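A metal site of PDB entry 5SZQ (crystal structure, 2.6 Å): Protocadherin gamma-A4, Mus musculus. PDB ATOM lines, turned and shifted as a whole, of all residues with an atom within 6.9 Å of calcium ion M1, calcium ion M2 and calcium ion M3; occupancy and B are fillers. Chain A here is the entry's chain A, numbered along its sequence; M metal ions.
Of the 26 residues printed, 6 come within 4 Å of calcium ion M1. The nearest printed residue that does not touch calcium ion M1 is Pro 212 (4.3 Å).
The side-chain carboxylate of Glu 176 sits close to the side-chain carboxylate of Asp 174. NH1 of Arg 175 lies close to OE2 of Glu 176. OD1 of Asp 207 lies close to NH1 of Arg 175 (3.8 Å). The side-chain carboxylate (OD2) of Asp 207 lies within hydrogen-bond range of the backbone NH (N) of Ser 244. OD1 of Asn 211 lies close to OD1 of Asp 210, 2.9 Å away. O of Val 206 sits at hydrogen-bond distance from N of Glu 121, at 3.4 Å. N of Leu 305 sits at hydrogen-bond distance from OD1 of Asp 299, 2.6 Å away. NH1 of Arg 175 sits close to O of Asp 243 (3.0 Å).
Along chain A the residues within 4 Å of calcium ion M3 span positions 121 to 211.
Calcium ion M1 is bound by the side-chain amide oxygen (OD1) of Asn 209 (2.4 Å), the backbone carbonyl oxygen (O) of Asn 211 (2.4 Å), the backbone carbonyl oxygen (O) of Asn 247 (2.4 Å), the side-chain carboxylate (OD2) of Asp 241 (2.5 Å), the side-chain carboxylate (OD2) of Asp 299 (2.6 Å) and the side-chain carboxylate (OD2) of Asp 243 (2.8 Å). Calcium ion M1 has six donor atoms within binding distance. Slightly farther from calcium ion M1 lies OD1 of Asp 241 (2.9 Å).
Calcium ion M3 is bound by OD2 of Asp 210 (2.5 Å), OD2 of Asp 174 (2.5 Å) and OE1 of Glu 121 (2.6 Å). Slightly farther from calcium ion M3 lies OE1 of Glu 176 (3.1 Å). Slightly farther from calcium ion M3 lies the side-chain carboxylate (OD1) of Asp 174 (3.1 Å).
Calcium ion M2 is bound by the side-chain carboxylate (OE2) of Glu 176, the side-chain carboxylate (OD1) of Asp 207, the backbone carbonyl oxygen (O) of Ile 208, the side-chain carboxylate (OE2) of Glu 121 and the side-chain carboxylate (OD1) of Asp 243. Slightly farther from calcium ion M2 lies OD1 of Asp 210 (3.0 Å). Slightly farther from calcium ion M2 lies OE1 of Glu 176 (3.0 Å).
Of the 26 residues printed, 6 come within 4 Å of calcium ion M2. The nearest printed residue that does not touch calcium ion M2 is Arg 175 (4.4 Å).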
ATOM      1  N   GLU A 121      37.021 -24.684 -28.865  1.00  0.00           N
ATOM      2  CA  GLU A 121      37.298 -24.119 -27.545  1.00  0.00           C
ATOM      3  C   GLU A 121      38.634 -24.619 -27.013  1.00  0.00           C
ATOM      4  O   GLU A 121      39.583 -23.837 -26.877  1.00  0.00           O
ATOM      5  CB  GLU A 121      36.151 -24.477 -26.587  1.00  0.00           C
ATOM      6  CG  GLU A 121      36.233 -23.769 -25.241  1.00  0.00           C
ATOM      7  CD  GLU A 121      35.072 -24.089 -24.325  1.00  0.00           C
ATOM      8  OE1 GLU A 121      35.319 -24.455 -23.160  1.00  0.00           O
ATOM      9  OE2 GLU A 121      33.910 -23.974 -24.780  1.00  0.00           O
ATOM     10  N   LEU A 173      42.311 -20.334 -25.965  1.00  0.00           N
ATOM     11  CA  LEU A 173      41.006 -19.716 -26.116  1.00  0.00           C
ATOM     12  C   LEU A 173      39.955 -20.531 -25.369  1.00  0.00           C
ATOM     13  O   LEU A 173      40.053 -21.758 -25.270  1.00  0.00           O
ATOM     14  CB  LEU A 173      40.647 -19.605 -27.603  1.00  0.00           C
ATOM     15  CG  LEU A 173      39.478 -18.719 -28.046  1.00  0.00           C
ATOM     16  CD1 LEU A 173      38.179 -19.488 -27.994  1.00  0.00           C
ATOM     17  CD2 LEU A 173      39.406 -17.445 -27.211  1.00  0.00           C
ATOM     18  N   ASP A 174      38.939 -19.840 -24.827  1.00  0.00           N
ATOM     19  CA  ASP A 174      37.859 -20.474 -24.077  1.00  0.00           C
ATOM     20  C   ASP A 174      36.557 -19.741 -24.376  1.00  0.00           C
ATOM     21  O   ASP A 174      36.476 -18.526 -24.171  1.00  0.00           O
ATOM     22  CB  ASP A 174      38.147 -20.465 -22.566  1.00  0.00           C
ATOM     23  CG  ASP A 174      37.036 -21.139 -21.751  1.00  0.00           C
ATOM     24  OD1 ASP A 174      36.966 -20.901 -20.522  1.00  0.00           O
ATOM     25  OD2 ASP A 174      36.247 -21.903 -22.343  1.00  0.00           O
ATOM     26  N   ARG A 175      35.556 -20.480 -24.836  1.00  0.00           N
ATOM     27  CA  ARG A 175      34.316 -19.863 -25.322  1.00  0.00           C
ATOM     28  C   ARG A 175      33.552 -19.160 -24.206  1.00  0.00           C
ATOM     29  O   ARG A 175      32.819 -18.200 -24.473  1.00  0.00           O
ATOM     30  CB  ARG A 175      33.447 -20.933 -25.984  1.00  0.00           C
ATOM     31  CG  ARG A 175      32.130 -20.442 -26.509  1.00  0.00           C
ATOM     32  CD  ARG A 175      31.011 -20.899 -25.601  1.00  0.00           C
ATOM     33  NE  ARG A 175      29.934 -19.920 -25.513  1.00  0.00           N
ATOM     34  CZ  ARG A 175      28.925 -19.991 -24.647  1.00  0.00           C
ATOM     35  NH1 ARG A 175      28.866 -21.002 -23.794  1.00  0.00           N
ATOM     36  NH2 ARG A 175      27.993 -19.050 -24.626  1.00  0.00           N
ATOM     37  N   GLU A 176      33.713 -19.598 -22.954  1.00  0.00           N
ATOM     38  CA  GLU A 176      32.926 -19.060 -21.852  1.00  0.00           C
ATOM     39  C   GLU A 176      33.301 -17.624 -21.475  1.00  0.00           C
ATOM     40  O   GLU A 176      32.657 -17.059 -20.594  1.00  0.00           O
ATOM     41  CB  GLU A 176      33.043 -19.965 -20.617  1.00  0.00           C
ATOM     42  CG  GLU A 176      32.150 -21.195 -20.659  1.00  0.00           C
ATOM     43  CD  GLU A 176      32.426 -22.082 -21.859  1.00  0.00           C
ATOM     44  OE1 GLU A 176      33.605 -22.403 -22.099  1.00  0.00           O
ATOM     45  OE2 GLU A 176      31.460 -22.431 -22.569  1.00  0.00           O
ATOM     46  N   GLU A 177      34.323 -17.034 -22.106  1.00  0.00           N
ATOM     47  CA  GLU A 177      34.683 -15.650 -21.832  1.00  0.00           C
ATOM     48  C   GLU A 177      33.946 -14.690 -22.767  1.00  0.00           C
ATOM     49  O   GLU A 177      33.244 -13.772 -22.307  1.00  0.00           O
ATOM     50  CB  GLU A 177      36.195 -15.448 -21.943  1.00  0.00           C
ATOM     51  CG  GLU A 177      36.978 -15.743 -20.669  1.00  0.00           C
ATOM     52  CD  GLU A 177      36.968 -17.217 -20.315  1.00  0.00           C
ATOM     53  OE1 GLU A 177      37.060 -17.541 -19.110  1.00  0.00           O
ATOM     54  OE2 GLU A 177      36.860 -18.052 -21.239  1.00  0.00           O
ATOM     55  N   VAL A 206      33.708 -22.104 -31.410  1.00  0.00           N
ATOM     56  CA  VAL A 206      33.104 -23.417 -31.173  1.00  0.00           C
ATOM     57  C   VAL A 206      33.025 -23.664 -29.673  1.00  0.00           C
ATOM     58  O   VAL A 206      33.916 -23.265 -28.905  1.00  0.00           O
ATOM     59  CB  VAL A 206      33.918 -24.510 -31.893  1.00  0.00           C
ATOM     60  CG1 VAL A 206      33.275 -25.868 -31.712  1.00  0.00           C
ATOM     61  CG2 VAL A 206      34.060 -24.167 -33.369  1.00  0.00           C
ATOM     62  N   ASP A 207      31.936 -24.311 -29.242  1.00  0.00           N
ATOM     63  CA  ASP A 207      31.611 -24.500 -27.834  1.00  0.00           C
ATOM     64  C   ASP A 207      31.667 -25.991 -27.499  1.00  0.00           C
ATOM     65  O   ASP A 207      30.833 -26.765 -27.979  1.00  0.00           O
ATOM     66  CB  ASP A 207      30.234 -23.921 -27.525  1.00  0.00           C
ATOM     67  CG  ASP A 207      29.745 -24.261 -26.137  1.00  0.00           C
ATOM     68  OD1 ASP A 207      30.541 -24.133 -25.183  1.00  0.00           O
ATOM     69  OD2 ASP A 207      28.574 -24.653 -25.983  1.00  0.00           O
ATOM     70  N   ILE A 208      32.656 -26.385 -26.680  1.00  0.00           N
ATOM     71  CA  ILE A 208      32.757 -27.753 -26.173  1.00  0.00           C
ATOM     72  C   ILE A 208      31.943 -27.858 -24.888  1.00  0.00           C
ATOM     73  O   ILE A 208      31.806 -26.897 -24.128  1.00  0.00           O
ATOM     74  CB  ILE A 208      34.232 -28.161 -25.926  1.00  0.00           C
ATOM     75  CG1 ILE A 208      35.038 -28.067 -27.217  1.00  0.00           C
ATOM     76  CG2 ILE A 208      34.330 -29.583 -25.366  1.00  0.00           C
ATOM     77  CD1 ILE A 208      36.423 -28.667 -27.092  1.00  0.00           C
ATOM     78  N   ASN A 209      31.381 -29.051 -24.654  1.00  0.00           N
ATOM     79  CA  ASN A 209      30.656 -29.338 -23.424  1.00  0.00           C
ATOM     80  C   ASN A 209      31.651 -29.757 -22.346  1.00  0.00           C
ATOM     81  O   ASN A 209      31.809 -30.935 -22.009  1.00  0.00           O
ATOM     82  CB  ASN A 209      29.615 -30.429 -23.671  1.00  0.00           C
ATOM     83  CG  ASN A 209      28.690 -30.640 -22.493  1.00  0.00           C
ATOM     84  OD1 ASN A 209      28.454 -29.717 -21.712  1.00  0.00           O
ATOM     85  ND2 ASN A 209      28.169 -31.856 -22.361  1.00  0.00           N
ATOM     86  N   ASP A 210      32.337 -28.763 -21.783  1.00  0.00           N
ATOM     87  CA  ASP A 210      33.358 -29.000 -20.766  1.00  0.00           C
ATOM     88  C   ASP A 210      32.961 -28.489 -19.389  1.00  0.00           C
ATOM     89  O   ASP A 210      33.709 -28.709 -18.432  1.00  0.00           O
ATOM     90  CB  ASP A 210      34.693 -28.370 -21.198  1.00  0.00           C
ATOM     91  CG  ASP A 210      34.616 -26.863 -21.333  1.00  0.00           C
ATOM     92  OD1 ASP A 210      33.498 -26.331 -21.496  1.00  0.00           O
ATOM     93  OD2 ASP A 210      35.682 -26.209 -21.291  1.00  0.00           O
ATOM     94  N   ASN A 211      31.815 -27.808 -19.259  1.00  0.00           N
ATOM     95  CA  ASN A 211      31.301 -27.364 -17.981  1.00  0.00           C
ATOM     96  C   ASN A 211      30.019 -28.114 -17.627  1.00  0.00           C
ATOM     97  O   ASN A 211      29.166 -28.318 -18.504  1.00  0.00           O
ATOM     98  CB  ASN A 211      31.021 -25.864 -17.975  1.00  0.00           C
ATOM     99  CG  ASN A 211      32.267 -25.024 -18.195  1.00  0.00           C
ATOM    100  OD1 ASN A 211      33.252 -25.499 -18.757  1.00  0.00           O
ATOM    101  ND2 ASN A 211      32.219 -23.772 -17.767  1.00  0.00           N
ATOM    102  N   PRO A 212      29.852 -28.554 -16.387  1.00  0.00           N
ATOM    103  CA  PRO A 212      28.598 -29.187 -15.985  1.00  0.00           C
ATOM    104  C   PRO A 212      27.609 -28.155 -15.471  1.00  0.00           C
ATOM    105  O   PRO A 212      27.983 -27.003 -15.211  1.00  0.00           O
ATOM    106  CB  PRO A 212      29.038 -30.137 -14.859  1.00  0.00           C
ATOM    107  CG  PRO A 212      30.195 -29.421 -14.238  1.00  0.00           C
ATOM    108  CD  PRO A 212      30.895 -28.688 -15.353  1.00  0.00           C
ATOM    109  N   PRO A 213      26.336 -28.525 -15.337  1.00  0.00           N
ATOM    110  CA  PRO A 213      25.369 -27.625 -14.678  1.00  0.00           C
ATOM    111  C   PRO A 213      25.605 -27.570 -13.179  1.00  0.00           C
ATOM    112  O   PRO A 213      25.782 -28.608 -12.529  1.00  0.00           O
ATOM    113  CB  PRO A 213      24.007 -28.243 -15.026  1.00  0.00           C
ATOM    114  CG  PRO A 213      24.308 -29.671 -15.346  1.00  0.00           C
ATOM    115  CD  PRO A 213      25.674 -29.689 -15.960  1.00  0.00           C
ATOM    116  N   ASP A 241      24.220 -23.788 -16.415  1.00  0.00           N
ATOM    117  CA  ASP A 241      25.337 -24.315 -17.170  1.00  0.00           C
ATOM    118  C   ASP A 241      25.965 -23.209 -18.005  1.00  0.00           C
ATOM    119  O   ASP A 241      25.291 -22.644 -18.885  1.00  0.00           O
ATOM    120  CB  ASP A 241      24.892 -25.470 -18.074  1.00  0.00           C
ATOM    121  CG  ASP A 241      26.068 -26.175 -18.736  1.00  0.00           C
ATOM    122  OD1 ASP A 241      27.061 -26.453 -18.020  1.00  0.00           O
ATOM    123  OD2 ASP A 241      26.019 -26.432 -19.948  1.00  0.00           O
ATOM    124  N   PRO A 242      27.238 -22.856 -17.777  1.00  0.00           N
ATOM    125  CA  PRO A 242      27.838 -21.718 -18.490  1.00  0.00           C
ATOM    126  C   PRO A 242      28.060 -21.960 -19.980  1.00  0.00           C
ATOM    127  O   PRO A 242      28.614 -21.075 -20.651  1.00  0.00           O
ATOM    128  CB  PRO A 242      29.181 -21.516 -17.765  1.00  0.00           C
ATOM    129  CG  PRO A 242      29.042 -22.236 -16.454  1.00  0.00           C
ATOM    130  CD  PRO A 242      28.131 -23.385 -16.734  1.00  0.00           C
ATOM    131  N   ASP A 243      27.662 -23.113 -20.528  1.00  0.00           N
ATOM    132  CA  ASP A 243      27.889 -23.394 -21.934  1.00  0.00           C
ATOM    133  C   ASP A 243      26.792 -22.777 -22.798  1.00  0.00           C
ATOM    134  O   ASP A 243      26.269 -21.710 -22.483  1.00  0.00           O
ATOM    135  CB  ASP A 243      27.978 -24.897 -22.183  1.00  0.00           C
ATOM    136  CG  ASP A 243      29.148 -25.544 -21.464  1.00  0.00           C
ATOM    137  OD1 ASP A 243      30.134 -24.820 -21.177  1.00  0.00           O
ATOM    138  OD2 ASP A 243      29.094 -26.757 -21.195  1.00  0.00           O
ATOM    139  N   SER A 244      26.441 -23.442 -23.896  1.00  0.00           N
ATOM    140  CA  SER A 244      25.454 -22.901 -24.820  1.00  0.00           C
ATOM    141  C   SER A 244      24.850 -24.047 -25.628  1.00  0.00           C
ATOM    142  O   SER A 244      25.419 -25.136 -25.720  1.00  0.00           O
ATOM    143  CB  SER A 244      26.073 -21.848 -25.745  1.00  0.00           C
ATOM    144  OG  SER A 244      25.093 -21.201 -26.532  1.00  0.00           O
ATOM    145  N   GLU A 246      22.754 -27.123 -27.051  1.00  0.00           N
ATOM    146  CA  GLU A 246      22.370 -28.392 -26.452  1.00  0.00           C
ATOM    147  C   GLU A 246      23.195 -28.694 -25.217  1.00  0.00           C
ATOM    148  O   GLU A 246      22.677 -29.192 -24.211  1.00  0.00           O
ATOM    149  CB  GLU A 246      22.502 -29.522 -27.482  1.00  0.00           C
ATOM    150  CG  GLU A 246      21.177 -30.103 -27.974  1.00  0.00           C
ATOM    151  CD  GLU A 246      21.378 -31.366 -28.778  1.00  0.00           C
ATOM    152  OE1 GLU A 246      22.514 -31.884 -28.808  1.00  0.00           O
ATOM    153  OE2 GLU A 246      20.407 -31.849 -29.402  1.00  0.00           O
ATOM    154  N   ASN A 247      24.488 -28.373 -25.252  1.00  0.00           N
ATOM    155  CA  ASN A 247      25.407 -28.634 -24.142  1.00  0.00           C
ATOM    156  C   ASN A 247      25.082 -27.850 -22.881  1.00  0.00           C
ATOM    157  O   ASN A 247      25.786 -28.013 -21.883  1.00  0.00           O
ATOM    158  CB  ASN A 247      26.838 -28.339 -24.588  1.00  0.00           C
ATOM    159  CG  ASN A 247      27.263 -29.166 -25.779  1.00  0.00           C
ATOM    160  OD1 ASN A 247      26.900 -30.336 -25.901  1.00  0.00           O
ATOM    161  ND2 ASN A 247      28.057 -28.572 -26.669  1.00  0.00           N
ATOM    162  N   ALA A 248      24.047 -27.009 -22.893  1.00  0.00           N
ATOM    163  CA  ALA A 248      23.729 -26.170 -21.739  1.00  0.00           C
ATOM    164  C   ALA A 248      22.307 -26.302 -21.230  1.00  0.00           C
ATOM    165  O   ALA A 248      21.981 -25.694 -20.204  1.00  0.00           O
ATOM    166  CB  ALA A 248      23.986 -24.692 -22.051  1.00  0.00           C
ATOM    167  N   GLN A 249      21.445 -27.058 -21.902  1.00  0.00           N
ATOM    168  CA  GLN A 249      20.126 -27.348 -21.365  1.00  0.00           C
ATOM    169  C   GLN A 249      20.245 -28.105 -20.053  1.00  0.00           C
ATOM    170  O   GLN A 249      21.212 -28.828 -19.822  1.00  0.00           O
ATOM    171  CB  GLN A 249      19.308 -28.171 -22.368  1.00  0.00           C
ATOM    172  CG  GLN A 249      19.109 -27.489 -23.718  1.00  0.00           C
ATOM    173  CD  GLN A 249      18.315 -28.359 -24.677  1.00  0.00           C
ATOM    174  OE1 GLN A 249      17.869 -29.449 -24.322  1.00  0.00           O
ATOM    175  NE2 GLN A 249      18.124 -27.871 -25.894  1.00  0.00           N
ATOM    176  N   ARG A 298      21.305 -32.894 -15.587  1.00  0.00           N
ATOM    177  CA  ARG A 298      22.174 -33.209 -16.713  1.00  0.00           C
ATOM    178  C   ARG A 298      21.933 -32.227 -17.859  1.00  0.00           C
ATOM    179  O   ARG A 298      21.056 -31.361 -17.786  1.00  0.00           O
ATOM    180  CB  ARG A 298      21.947 -34.656 -17.181  1.00  0.00           C
ATOM    181  CG  ARG A 298      20.578 -34.904 -17.806  1.00  0.00           C
ATOM    182  CD  ARG A 298      20.493 -36.302 -18.409  1.00  0.00           C
ATOM    183  NE  ARG A 298      19.175 -36.566 -18.978  1.00  0.00           N
ATOM    184  CZ  ARG A 298      18.827 -36.278 -20.227  1.00  0.00           C
ATOM    185  NH1 ARG A 298      17.599 -36.549 -20.663  1.00  0.00           N
ATOM    186  NH2 ARG A 298      19.701 -35.718 -21.053  1.00  0.00           N
ATOM    187  N   ASP A 299      22.732 -32.359 -18.920  1.00  0.00           N
ATOM    188  CA  ASP A 299      22.564 -31.579 -20.134  1.00  0.00           C
ATOM    189  C   ASP A 299      22.294 -32.504 -21.313  1.00  0.00           C
ATOM    190  O   ASP A 299      22.509 -33.718 -21.246  1.00  0.00           O
ATOM    191  CB  ASP A 299      23.786 -30.686 -20.420  1.00  0.00           C
ATOM    192  CG  ASP A 299      25.081 -31.470 -20.598  1.00  0.00           C
ATOM    193  OD1 ASP A 299      25.065 -32.710 -20.559  1.00  0.00           O
ATOM    194  OD2 ASP A 299      26.136 -30.820 -20.781  1.00  0.00           O
ATOM    195  N   SER A 300      21.799 -31.911 -22.396  1.00  0.00           N
ATOM    196  CA  SER A 300      21.510 -32.665 -23.615  1.00  0.00           C
ATOM    197  C   SER A 300      22.806 -32.885 -24.390  1.00  0.00           C
ATOM    198  O   SER A 300      23.905 -32.599 -23.921  1.00  0.00           O
ATOM    199  CB  SER A 300      20.444 -31.941 -24.434  1.00  0.00           C
ATOM    200  OG  SER A 300      19.259 -31.743 -23.680  1.00  0.00           O
ATOM    201  N   LEU A 305      26.337 -34.514 -19.260  1.00  0.00           N
ATOM    202  CA  LEU A 305      27.164 -34.098 -18.139  1.00  0.00           C
ATOM    203  C   LEU A 305      26.250 -33.554 -17.050  1.00  0.00           C
ATOM    204  O   LEU A 305      25.484 -32.615 -17.293  1.00  0.00           O
ATOM    205  CB  LEU A 305      28.173 -33.028 -18.569  1.00  0.00           C
ATOM    206  CG  LEU A 305      29.164 -32.477 -17.537  1.00  0.00           C
ATOM    207  CD1 LEU A 305      29.832 -33.591 -16.748  1.00  0.00           C
ATOM    208  CD2 LEU A 305      30.218 -31.596 -18.206  1.00  0.00           C
HETATM  209 CA    CA M   1      27.281 -28.566 -20.024  1.00  0.00          CA
HETATM  210 CA    CA M   2      31.877 -24.583 -23.327  1.00  0.00          CA
HETATM  211 CA    CA M   3      35.940 -23.831 -20.713  1.00  0.00          CA
